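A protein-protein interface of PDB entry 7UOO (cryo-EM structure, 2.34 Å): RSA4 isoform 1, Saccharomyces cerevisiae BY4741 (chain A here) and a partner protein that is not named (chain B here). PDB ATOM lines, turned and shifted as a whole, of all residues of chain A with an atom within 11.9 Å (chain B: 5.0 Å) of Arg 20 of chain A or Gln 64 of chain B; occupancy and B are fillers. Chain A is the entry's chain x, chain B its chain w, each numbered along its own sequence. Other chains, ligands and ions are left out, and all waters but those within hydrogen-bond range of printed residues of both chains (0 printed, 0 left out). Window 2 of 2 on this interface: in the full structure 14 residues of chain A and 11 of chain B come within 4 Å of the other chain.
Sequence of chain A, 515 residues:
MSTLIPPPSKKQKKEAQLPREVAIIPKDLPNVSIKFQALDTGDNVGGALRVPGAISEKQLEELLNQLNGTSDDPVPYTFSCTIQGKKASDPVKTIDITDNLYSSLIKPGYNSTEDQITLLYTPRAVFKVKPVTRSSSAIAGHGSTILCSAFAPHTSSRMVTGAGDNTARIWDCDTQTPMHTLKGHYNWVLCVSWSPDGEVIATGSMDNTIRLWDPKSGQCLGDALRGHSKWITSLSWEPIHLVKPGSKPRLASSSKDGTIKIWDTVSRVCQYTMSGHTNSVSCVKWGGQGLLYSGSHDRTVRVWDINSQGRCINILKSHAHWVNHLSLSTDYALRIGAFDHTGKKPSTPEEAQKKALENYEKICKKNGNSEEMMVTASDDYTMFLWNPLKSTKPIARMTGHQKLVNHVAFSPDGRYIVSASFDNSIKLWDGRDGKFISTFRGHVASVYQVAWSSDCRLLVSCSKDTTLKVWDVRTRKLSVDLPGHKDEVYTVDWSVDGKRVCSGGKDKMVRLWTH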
ATOM      1  N   LYS A  11       8.062   7.387 -12.906  1.00  0.00           N
ATOM      2  CA  LYS A  11       6.997   7.282 -11.915  1.00  0.00           C
ATOM      3  C   LYS A  11       5.651   7.652 -12.518  1.00  0.00           C
ATOM      4  O   LYS A  11       4.630   7.028 -12.210  1.00  0.00           O
ATOM      5  CB  LYS A  11       7.308   8.172 -10.712  1.00  0.00           C
ATOM      6  CG  LYS A  11       8.722   8.027 -10.180  1.00  0.00           C
ATOM      7  CD  LYS A  11       8.887   8.742  -8.850  1.00  0.00           C
ATOM      8  CE  LYS A  11      10.351   8.843  -8.455  1.00  0.00           C
ATOM      9  NZ  LYS A  11      11.012   7.512  -8.409  1.00  0.00           N
ATOM     10  N   GLN A  12       5.631   8.664 -13.385  1.00  0.00           N
ATOM     11  CA  GLN A  12       4.388   9.061 -14.039  1.00  0.00           C
ATOM     12  C   GLN A  12       3.896   7.985 -15.000  1.00  0.00           C
ATOM     13  O   GLN A  12       2.687   7.759 -15.120  1.00  0.00           O
ATOM     14  CB  GLN A  12       4.589  10.392 -14.757  1.00  0.00           C
ATOM     15  CG  GLN A  12       4.977  11.523 -13.816  1.00  0.00           C
ATOM     16  CD  GLN A  12       5.460  12.757 -14.546  1.00  0.00           C
ATOM     17  OE1 GLN A  12       6.403  12.696 -15.333  1.00  0.00           O
ATOM     18  NE2 GLN A  12       4.810  13.887 -14.290  1.00  0.00           N
ATOM     19  N   LYS A  13       4.816   7.307 -15.689  1.00  0.00           N
ATOM     20  CA  LYS A  13       4.420   6.192 -16.546  1.00  0.00           C
ATOM     21  C   LYS A  13       3.839   5.045 -15.727  1.00  0.00           C
ATOM     22  O   LYS A  13       2.857   4.413 -16.138  1.00  0.00           O
ATOM     23  CB  LYS A  13       5.612   5.718 -17.373  1.00  0.00           C
ATOM     24  CG  LYS A  13       5.763   6.444 -18.697  1.00  0.00           C
ATOM     25  CD  LYS A  13       7.124   6.191 -19.316  1.00  0.00           C
ATOM     26  CE  LYS A  13       7.056   6.291 -20.830  1.00  0.00           C
ATOM     27  NZ  LYS A  13       6.154   7.393 -21.268  1.00  0.00           N
ATOM     28  N   LYS A  14       4.430   4.764 -14.563  1.00  0.00           N
ATOM     29  CA  LYS A  14       3.866   3.745 -13.680  1.00  0.00           C
ATOM     30  C   LYS A  14       2.480   4.147 -13.180  1.00  0.00           C
ATOM     31  O   LYS A  14       1.570   3.309 -13.101  1.00  0.00           O
ATOM     32  CB  LYS A  14       4.810   3.487 -12.508  1.00  0.00           C
ATOM     33  CG  LYS A  14       6.139   2.876 -12.910  1.00  0.00           C
ATOM     34  CD  LYS A  14       5.957   1.470 -13.456  1.00  0.00           C
ATOM     35  CE  LYS A  14       5.397   0.541 -12.392  1.00  0.00           C
ATOM     36  NZ  LYS A  14       6.243   0.548 -11.169  1.00  0.00           N
ATOM     37  N   GLU A  15       2.301   5.427 -12.840  1.00  0.00           N
ATOM     38  CA  GLU A  15       0.988   5.913 -12.425  1.00  0.00           C
ATOM     39  C   GLU A  15      -0.035   5.760 -13.544  1.00  0.00           C
ATOM     40  O   GLU A  15      -1.192   5.407 -13.294  1.00  0.00           O
ATOM     41  CB  GLU A  15       1.076   7.375 -11.986  1.00  0.00           C
ATOM     42  CG  GLU A  15       1.875   7.616 -10.717  1.00  0.00           C
ATOM     43  CD  GLU A  15       2.155   9.091 -10.479  1.00  0.00           C
ATOM     44  OE1 GLU A  15       1.329   9.929 -10.898  1.00  0.00           O
ATOM     45  OE2 GLU A  15       3.206   9.415  -9.885  1.00  0.00           O
ATOM     46  N   ALA A  16       0.375   6.039 -14.785  1.00  0.00           N
ATOM     47  CA  ALA A  16      -0.523   5.864 -15.923  1.00  0.00           C
ATOM     48  C   ALA A  16      -0.890   4.399 -16.118  1.00  0.00           C
ATOM     49  O   ALA A  16      -2.044   4.075 -16.424  1.00  0.00           O
ATOM     50  CB  ALA A  16       0.119   6.431 -17.188  1.00  0.00           C
ATOM     51  N   GLN A  17       0.079   3.496 -15.948  1.00  0.00           N
ATOM     52  CA  GLN A  17      -0.204   2.073 -16.098  1.00  0.00           C
ATOM     53  C   GLN A  17      -1.024   1.516 -14.941  1.00  0.00           C
ATOM     54  O   GLN A  17      -1.603   0.433 -15.075  1.00  0.00           O
ATOM     55  CB  GLN A  17       1.100   1.290 -16.242  1.00  0.00           C
ATOM     56  CG  GLN A  17       1.820   1.554 -17.549  1.00  0.00           C
ATOM     57  CD  GLN A  17       3.172   0.881 -17.614  1.00  0.00           C
ATOM     58  OE1 GLN A  17       3.768   0.763 -18.684  1.00  0.00           O
ATOM     59  NE2 GLN A  17       3.670   0.441 -16.465  1.00  0.00           N
ATOM     60  N   LEU A  18      -1.076   2.224 -13.815  1.00  0.00           N
ATOM     61  CA  LEU A  18      -1.971   1.839 -12.733  1.00  0.00           C
ATOM     62  C   LEU A  18      -3.427   1.919 -13.198  1.00  0.00           C
ATOM     63  O   LEU A  18      -3.762   2.728 -14.068  1.00  0.00           O
ATOM     64  CB  LEU A  18      -1.757   2.741 -11.517  1.00  0.00           C
ATOM     65  CG  LEU A  18      -0.559   2.395 -10.634  1.00  0.00           C
ATOM     66  CD1 LEU A  18      -0.427   3.382  -9.485  1.00  0.00           C
ATOM     67  CD2 LEU A  18      -0.685   0.972 -10.112  1.00  0.00           C
ATOM     68  N   PRO A  19      -4.309   1.074 -12.653  1.00  0.00           N
ATOM     69  CA  PRO A  19      -5.705   1.069 -13.113  1.00  0.00           C
ATOM     70  C   PRO A  19      -6.421   2.375 -12.797  1.00  0.00           C
ATOM     71  O   PRO A  19      -6.158   3.032 -11.788  1.00  0.00           O
ATOM     72  CB  PRO A  19      -6.327  -0.108 -12.350  1.00  0.00           C
ATOM     73  CG  PRO A  19      -5.452  -0.297 -11.165  1.00  0.00           C
ATOM     74  CD  PRO A  19      -4.068   0.047 -11.624  1.00  0.00           C
ATOM     75  N   ARG A  20      -7.345   2.740 -13.680  1.00  0.00           N
ATOM     76  CA  ARG A  20      -8.045   4.012 -13.607  1.00  0.00           C
ATOM     77  C   ARG A  20      -9.350   3.876 -12.831  1.00  0.00           C
ATOM     78  O   ARG A  20      -9.887   2.780 -12.647  1.00  0.00           O
ATOM     79  CB  ARG A  20      -8.333   4.548 -15.011  1.00  0.00           C
ATOM     80  CG  ARG A  20      -7.095   4.854 -15.843  1.00  0.00           C
ATOM     81  CD  ARG A  20      -6.410   6.129 -15.381  1.00  0.00           C
ATOM     82  NE  ARG A  20      -7.362   7.216 -15.195  1.00  0.00           N
ATOM     83  CZ  ARG A  20      -7.028   8.489 -15.034  1.00  0.00           C
ATOM     84  NH1 ARG A  20      -5.764   8.881 -15.066  1.00  0.00           N
ATOM     85  NH2 ARG A  20      -7.985   9.392 -14.840  1.00  0.00           N
ATOM     86  N   GLU A  21      -9.862   5.016 -12.379  1.00  0.00           N
ATOM     87  CA  GLU A  21     -11.137   5.083 -11.683  1.00  0.00           C
ATOM     88  C   GLU A  21     -12.237   5.465 -12.666  1.00  0.00           C
ATOM     89  O   GLU A  21     -12.020   6.273 -13.573  1.00  0.00           O
ATOM     90  CB  GLU A  21     -11.079   6.084 -10.526  1.00  0.00           C
ATOM     91  CG  GLU A  21     -10.505   7.446 -10.886  1.00  0.00           C
ATOM     92  CD  GLU A  21     -11.555   8.407 -11.411  1.00  0.00           C
ATOM     93  OE1 GLU A  21     -12.647   8.486 -10.808  1.00  0.00           O
ATOM     94  OE2 GLU A  21     -11.292   9.071 -12.437  1.00  0.00           O
ATOM     95  N   VAL A  22     -13.413   4.873 -12.486  1.00  0.00           N
ATOM     96  CA  VAL A  22     -14.541   5.065 -13.389  1.00  0.00           C
ATOM     97  C   VAL A  22     -15.547   5.977 -12.704  1.00  0.00           C
ATOM     98  O   VAL A  22     -16.062   5.649 -11.627  1.00  0.00           O
ATOM     99  CB  VAL A  22     -15.184   3.727 -13.781  1.00  0.00           C
ATOM    100  CG1 VAL A  22     -16.239   3.940 -14.847  1.00  0.00           C
ATOM    101  CG2 VAL A  22     -14.125   2.754 -14.263  1.00  0.00           C
ATOM    102  N   ALA A  23     -15.829   7.120 -13.328  1.00  0.00           N
ATOM    103  CA  ALA A  23     -16.796   8.065 -12.783  1.00  0.00           C
ATOM    104  C   ALA A  23     -18.210   7.536 -12.969  1.00  0.00           C
ATOM    105  O   ALA A  23     -18.829   7.753 -14.016  1.00  0.00           O
ATOM    106  CB  ALA A  23     -16.644   9.435 -13.445  1.00  0.00           C
ATOM    107  N   ILE A  24     -18.726   6.842 -11.961  1.00  0.00           N
ATOM    108  CA  ILE A  24     -20.040   6.219 -12.026  1.00  0.00           C
ATOM    109  C   ILE A  24     -20.976   6.957 -11.079  1.00  0.00           C
ATOM    110  O   ILE A  24     -20.548   7.557 -10.087  1.00  0.00           O
ATOM    111  CB  ILE A  24     -19.963   4.712 -11.694  1.00  0.00           C
ATOM    112  CG1 ILE A  24     -21.199   3.977 -12.212  1.00  0.00           C
ATOM    113  CG2 ILE A  24     -19.780   4.485 -10.201  1.00  0.00           C
ATOM    114  CD1 ILE A  24     -21.366   4.048 -13.712  1.00  0.00           C
ATOM    115  N   LYS A 107     -19.435  15.733  -6.542  1.00  0.00           N
ATOM    116  CA  LYS A 107     -18.147  15.084  -6.782  1.00  0.00           C
ATOM    117  C   LYS A 107     -16.948  15.957  -6.408  1.00  0.00           C
ATOM    118  O   LYS A 107     -16.006  15.418  -5.799  1.00  0.00           O
ATOM    119  CB  LYS A 107     -18.059  14.608  -8.240  1.00  0.00           C
ATOM    120  CG  LYS A 107     -16.720  13.987  -8.610  1.00  0.00           C
ATOM    121  CD  LYS A 107     -16.646  13.662 -10.090  1.00  0.00           C
ATOM    122  CE  LYS A 107     -15.237  13.260 -10.497  1.00  0.00           C
ATOM    123  NZ  LYS A 107     -15.118  13.073 -11.970  1.00  0.00           N
ATOM    124  N   TYR B  21      -5.901  -5.187 -16.803  1.00  0.00           N
ATOM    125  CA  TYR B  21      -5.950  -4.456 -18.058  1.00  0.00           C
ATOM    126  C   TYR B  21      -4.545  -4.191 -18.573  1.00  0.00           C
ATOM    127  O   TYR B  21      -3.612  -3.962 -17.799  1.00  0.00           O
ATOM    128  CB  TYR B  21      -6.684  -3.115 -17.905  1.00  0.00           C
ATOM    129  CG  TYR B  21      -8.065  -3.216 -17.308  1.00  0.00           C
ATOM    130  CD1 TYR B  21      -9.147  -3.619 -18.076  1.00  0.00           C
ATOM    131  CD2 TYR B  21      -8.291  -2.890 -15.977  1.00  0.00           C
ATOM    132  CE1 TYR B  21     -10.413  -3.705 -17.537  1.00  0.00           C
ATOM    133  CE2 TYR B  21      -9.553  -2.973 -15.426  1.00  0.00           C
ATOM    134  CZ  TYR B  21     -10.611  -3.380 -16.211  1.00  0.00           C
ATOM    135  OH  TYR B  21     -11.873  -3.466 -15.668  1.00  0.00           O
ATOM    136  N   LEU B  23      -3.963  -1.490 -21.246  1.00  0.00           N
ATOM    137  CA  LEU B  23      -4.592  -0.508 -22.122  1.00  0.00           C
ATOM    138  C   LEU B  23      -3.697  -0.115 -23.290  1.00  0.00           C
ATOM    139  O   LEU B  23      -4.204   0.392 -24.296  1.00  0.00           O
ATOM    140  CB  LEU B  23      -4.989   0.730 -21.319  1.00  0.00           C
ATOM    141  CG  LEU B  23      -5.956   0.469 -20.162  1.00  0.00           C
ATOM    142  CD1 LEU B  23      -6.325   1.761 -19.456  1.00  0.00           C
ATOM    143  CD2 LEU B  23      -7.201  -0.249 -20.653  1.00  0.00           C
ATOM    144  N   LEU B  60     -16.089  -3.464 -19.376  1.00  0.00           N
ATOM    145  CA  LEU B  60     -15.052  -3.019 -18.445  1.00  0.00           C
ATOM    146  C   LEU B  60     -13.907  -2.315 -19.173  1.00  0.00           C
ATOM    147  O   LEU B  60     -13.424  -1.260 -18.728  1.00  0.00           O
ATOM    148  CB  LEU B  60     -14.523  -4.208 -17.643  1.00  0.00           C
ATOM    149  CG  LEU B  60     -15.510  -4.908 -16.709  1.00  0.00           C
ATOM    150  CD1 LEU B  60     -14.836  -6.067 -15.996  1.00  0.00           C
ATOM    151  CD2 LEU B  60     -16.085  -3.925 -15.707  1.00  0.00           C
ATOM    152  N   LEU B  61     -13.471  -2.880 -20.301  1.00  0.00           N
ATOM    153  CA  LEU B  61     -12.372  -2.285 -21.058  1.00  0.00           C
ATOM    154  C   LEU B  61     -12.751  -0.912 -21.604  1.00  0.00           C
ATOM    155  O   LEU B  61     -11.936   0.017 -21.587  1.00  0.00           O
ATOM    156  CB  LEU B  61     -11.957  -3.219 -22.194  1.00  0.00           C
ATOM    157  CG  LEU B  61     -10.763  -2.778 -23.038  1.00  0.00           C
ATOM    158  CD1 LEU B  61      -9.485  -2.804 -22.217  1.00  0.00           C
ATOM    159  CD2 LEU B  61     -10.631  -3.650 -24.273  1.00  0.00           C
ATOM    160  N   ILE B  62     -13.986  -0.768 -22.088  1.00  0.00           N
ATOM    161  CA  ILE B  62     -14.452   0.513 -22.605  1.00  0.00           C
ATOM    162  C   ILE B  62     -14.554   1.539 -21.484  1.00  0.00           C
ATOM    163  O   ILE B  62     -14.232   2.717 -21.678  1.00  0.00           O
ATOM    164  CB  ILE B  62     -15.792   0.327 -23.345  1.00  0.00           C
ATOM    165  CG1 ILE B  62     -15.564  -0.368 -24.687  1.00  0.00           C
ATOM    166  CG2 ILE B  62     -16.494   1.658 -23.571  1.00  0.00           C
ATOM    167  CD1 ILE B  62     -14.707   0.425 -25.643  1.00  0.00           C
ATOM    168  N   ASN B  63     -14.989   1.110 -20.295  1.00  0.00           N
ATOM    169  CA  ASN B  63     -15.008   2.011 -19.146  1.00  0.00           C
ATOM    170  C   ASN B  63     -13.610   2.538 -18.842  1.00  0.00           C
ATOM    171  O   ASN B  63     -13.415   3.746 -18.652  1.00  0.00           O
ATOM    172  CB  ASN B  63     -15.587   1.293 -17.925  1.00  0.00           C
ATOM    173  CG  ASN B  63     -17.069   1.003 -18.062  1.00  0.00           C
ATOM    174  OD1 ASN B  63     -17.658   1.196 -19.124  1.00  0.00           O
ATOM    175  ND2 ASN B  63     -17.679   0.529 -16.982  1.00  0.00           N
ATOM    176  N   GLN B  64     -12.616   1.643 -18.825  1.00  0.00           N
ATOM    177  CA  GLN B  64     -11.241   2.077 -18.577  1.00  0.00           C
ATOM    178  C   GLN B  64     -10.746   3.029 -19.664  1.00  0.00           C
ATOM    179  O   GLN B  64     -10.145   4.073 -19.365  1.00  0.00           O
ATOM    180  CB  GLN B  64     -10.318   0.861 -18.472  1.00  0.00           C
ATOM    181  CG  GLN B  64     -10.657  -0.090 -17.338  1.00  0.00           C
ATOM    182  CD  GLN B  64     -10.405   0.509 -15.970  1.00  0.00           C
ATOM    183  OE1 GLN B  64      -9.268   0.569 -15.507  1.00  0.00           O
ATOM    184  NE2 GLN B  64     -11.468   0.958 -15.316  1.00  0.00           N
ATOM    185  N   LEU B  65     -11.005   2.693 -20.932  1.00  0.00           N
ATOM    186  CA  LEU B  65     -10.514   3.513 -22.037  1.00  0.00           C
ATOM    187  C   LEU B  65     -11.146   4.898 -22.032  1.00  0.00           C
ATOM    188  O   LEU B  65     -10.462   5.899 -22.273  1.00  0.00           O
ATOM    189  CB  LEU B  65     -10.777   2.811 -23.369  1.00  0.00           C
ATOM    190  CG  LEU B  65      -9.941   1.562 -23.645  1.00  0.00           C
ATOM    191  CD1 LEU B  65     -10.281   0.973 -25.004  1.00  0.00           C
ATOM    192  CD2 LEU B  65      -8.460   1.878 -23.546  1.00  0.00           C
ATOM    193  N   LEU B  66     -12.446   4.982 -21.758  1.00  0.00           N
ATOM    194  CA  LEU B  66     -13.113   6.275 -21.734  1.00  0.00           C
ATOM    195  C   LEU B  66     -12.874   7.038 -20.440  1.00  0.00           C
ATOM    196  O   LEU B  66     -13.186   8.231 -20.380  1.00  0.00           O
ATOM    197  CB  LEU B  66     -14.615   6.099 -21.976  1.00  0.00           C
ATOM    198  CG  LEU B  66     -14.982   5.542 -23.355  1.00  0.00           C
ATOM    199  CD1 LEU B  66     -16.479   5.600 -23.592  1.00  0.00           C
ATOM    200  CD2 LEU B  66     -14.238   6.281 -24.454  1.00  0.00           C
ATOM    201  N   SER B  67     -12.338   6.388 -19.406  1.00  0.00           N
ATOM    202  CA  SER B  67     -11.848   7.115 -18.245  1.00  0.00           C
ATOM    203  C   SER B  67     -10.376   7.497 -18.360  1.00  0.00           C
ATOM    204  O   SER B  67      -9.875   8.225 -17.498  1.00  0.00           O
ATOM    205  CB  SER B  67     -12.064   6.292 -16.972  1.00  0.00           C
ATOM    206  OG  SER B  67     -13.444   6.064 -16.751  1.00  0.00           O
ATOM    207  N   LEU B  68      -9.680   7.023 -19.393  1.00  0.00           N
ATOM    208  CA  LEU B  68      -8.307   7.450 -19.631  1.00  0.00           C
ATOM    209  C   LEU B  68      -8.250   8.948 -19.942  1.00  0.00           C
ATOM    210  O   LEU B  68      -9.235   9.530 -20.406  1.00  0.00           O
ATOM    211  CB  LEU B  68      -7.697   6.664 -20.789  1.00  0.00           C
ATOM    212  CG  LEU B  68      -7.044   5.320 -20.479  1.00  0.00           C
ATOM    213  CD1 LEU B  68      -6.526   4.712 -21.762  1.00  0.00           C
ATOM    214  CD2 LEU B  68      -5.919   5.484 -19.472  1.00  0.00           C
ATOM    215  N   PRO B  69      -7.115   9.599 -19.687  1.00  0.00           N
ATOM    216  CA  PRO B  69      -6.986  11.022 -20.024  1.00  0.00           C
ATOM    217  C   PRO B  69      -7.046  11.262 -21.525  1.00  0.00           C
ATOM    218  O   PRO B  69      -6.747  10.389 -22.344  1.00  0.00           O
ATOM    219  CB  PRO B  69      -5.614  11.405 -19.456  1.00  0.00           C
ATOM    220  CG  PRO B  69      -4.885  10.117 -19.312  1.00  0.00           C
ATOM    221  CD  PRO B  69      -5.931   9.110 -18.959  1.00  0.00           C
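Gln 64 of chain B touches two residues of chain A.
No residue of chain A comes within 4 Å of Tyr 21 of chain B.
No residue of chain A comes within 4 Å of Ile 62 of chain B.
No residue of chain A comes within 4 Å of Asn 63 of chain B.
Leu 65 of chain B touches none of the printed residues of chain A.
Of chain A, only Arg 20, Glu 21 and Val 22 come within 4 Å of Ser 67 of chain B.
Pro 69 of chain B touches just one residue of chain A: Arg 20 (3.9 Å).
Of the printed residues of chain B, Val 22 of chain A touches Gln 64 (3.4 Å) and Ser 67 (3.7 Å).
Printed residues of chain B within 4 Å of Glu 21 of chain A: Ser 67.
The nearest residue of chain A that does not touch Gln 64 of chain B is Pro 19 of chain A (4.3 Å).
The guanidinium group (NH2) of Arg 20 of chain A sits at hydrogen-bond distance from the backbone carbonyl oxygen (O) of Ser 67 of chain B, at 3.5 Å.
OG of Ser 67 of chain B sits close to O of Glu 21 of chain A (3.5 Å).
The side-chain amide oxygen of Gln 64 of chain B lies within hydrogen-bond range of the backbone NH of Arg 20 of chain A, 3.4 Å away.
OG of Ser 67 of chain B lies within hydrogen-bond range of O of Asn 63 of chain B.
Printed residues of chain A that touch a printed residue of chain B: Arg 20, Glu 21 and Val 22.
Of the 12 printed residues of chain B, 4 touch a printed residue of chain A.
Hydrophobic or aromatic side chains of chain B within 4 Å of the printed part of chain A: Leu 68 and Pro 69.
Among the printed residues, 7 pairs touch across the chains.
Among the printed residues, no Asp or Glu carboxylate lies within 4 Å of a Lys or Arg side-chain nitrogen of the other chain.
Arg 20 of chain A touches Leu 68 of chain B.
Arg 20 of chain A touches Pro 69 of chain B (NH1 to CD, 3.9 Å).
Val 22 of chain A touches Gln 64 of chain B.
OG of Ser 67 of chain B touches CA of Val 22 of chain A, at 3.7 Å.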
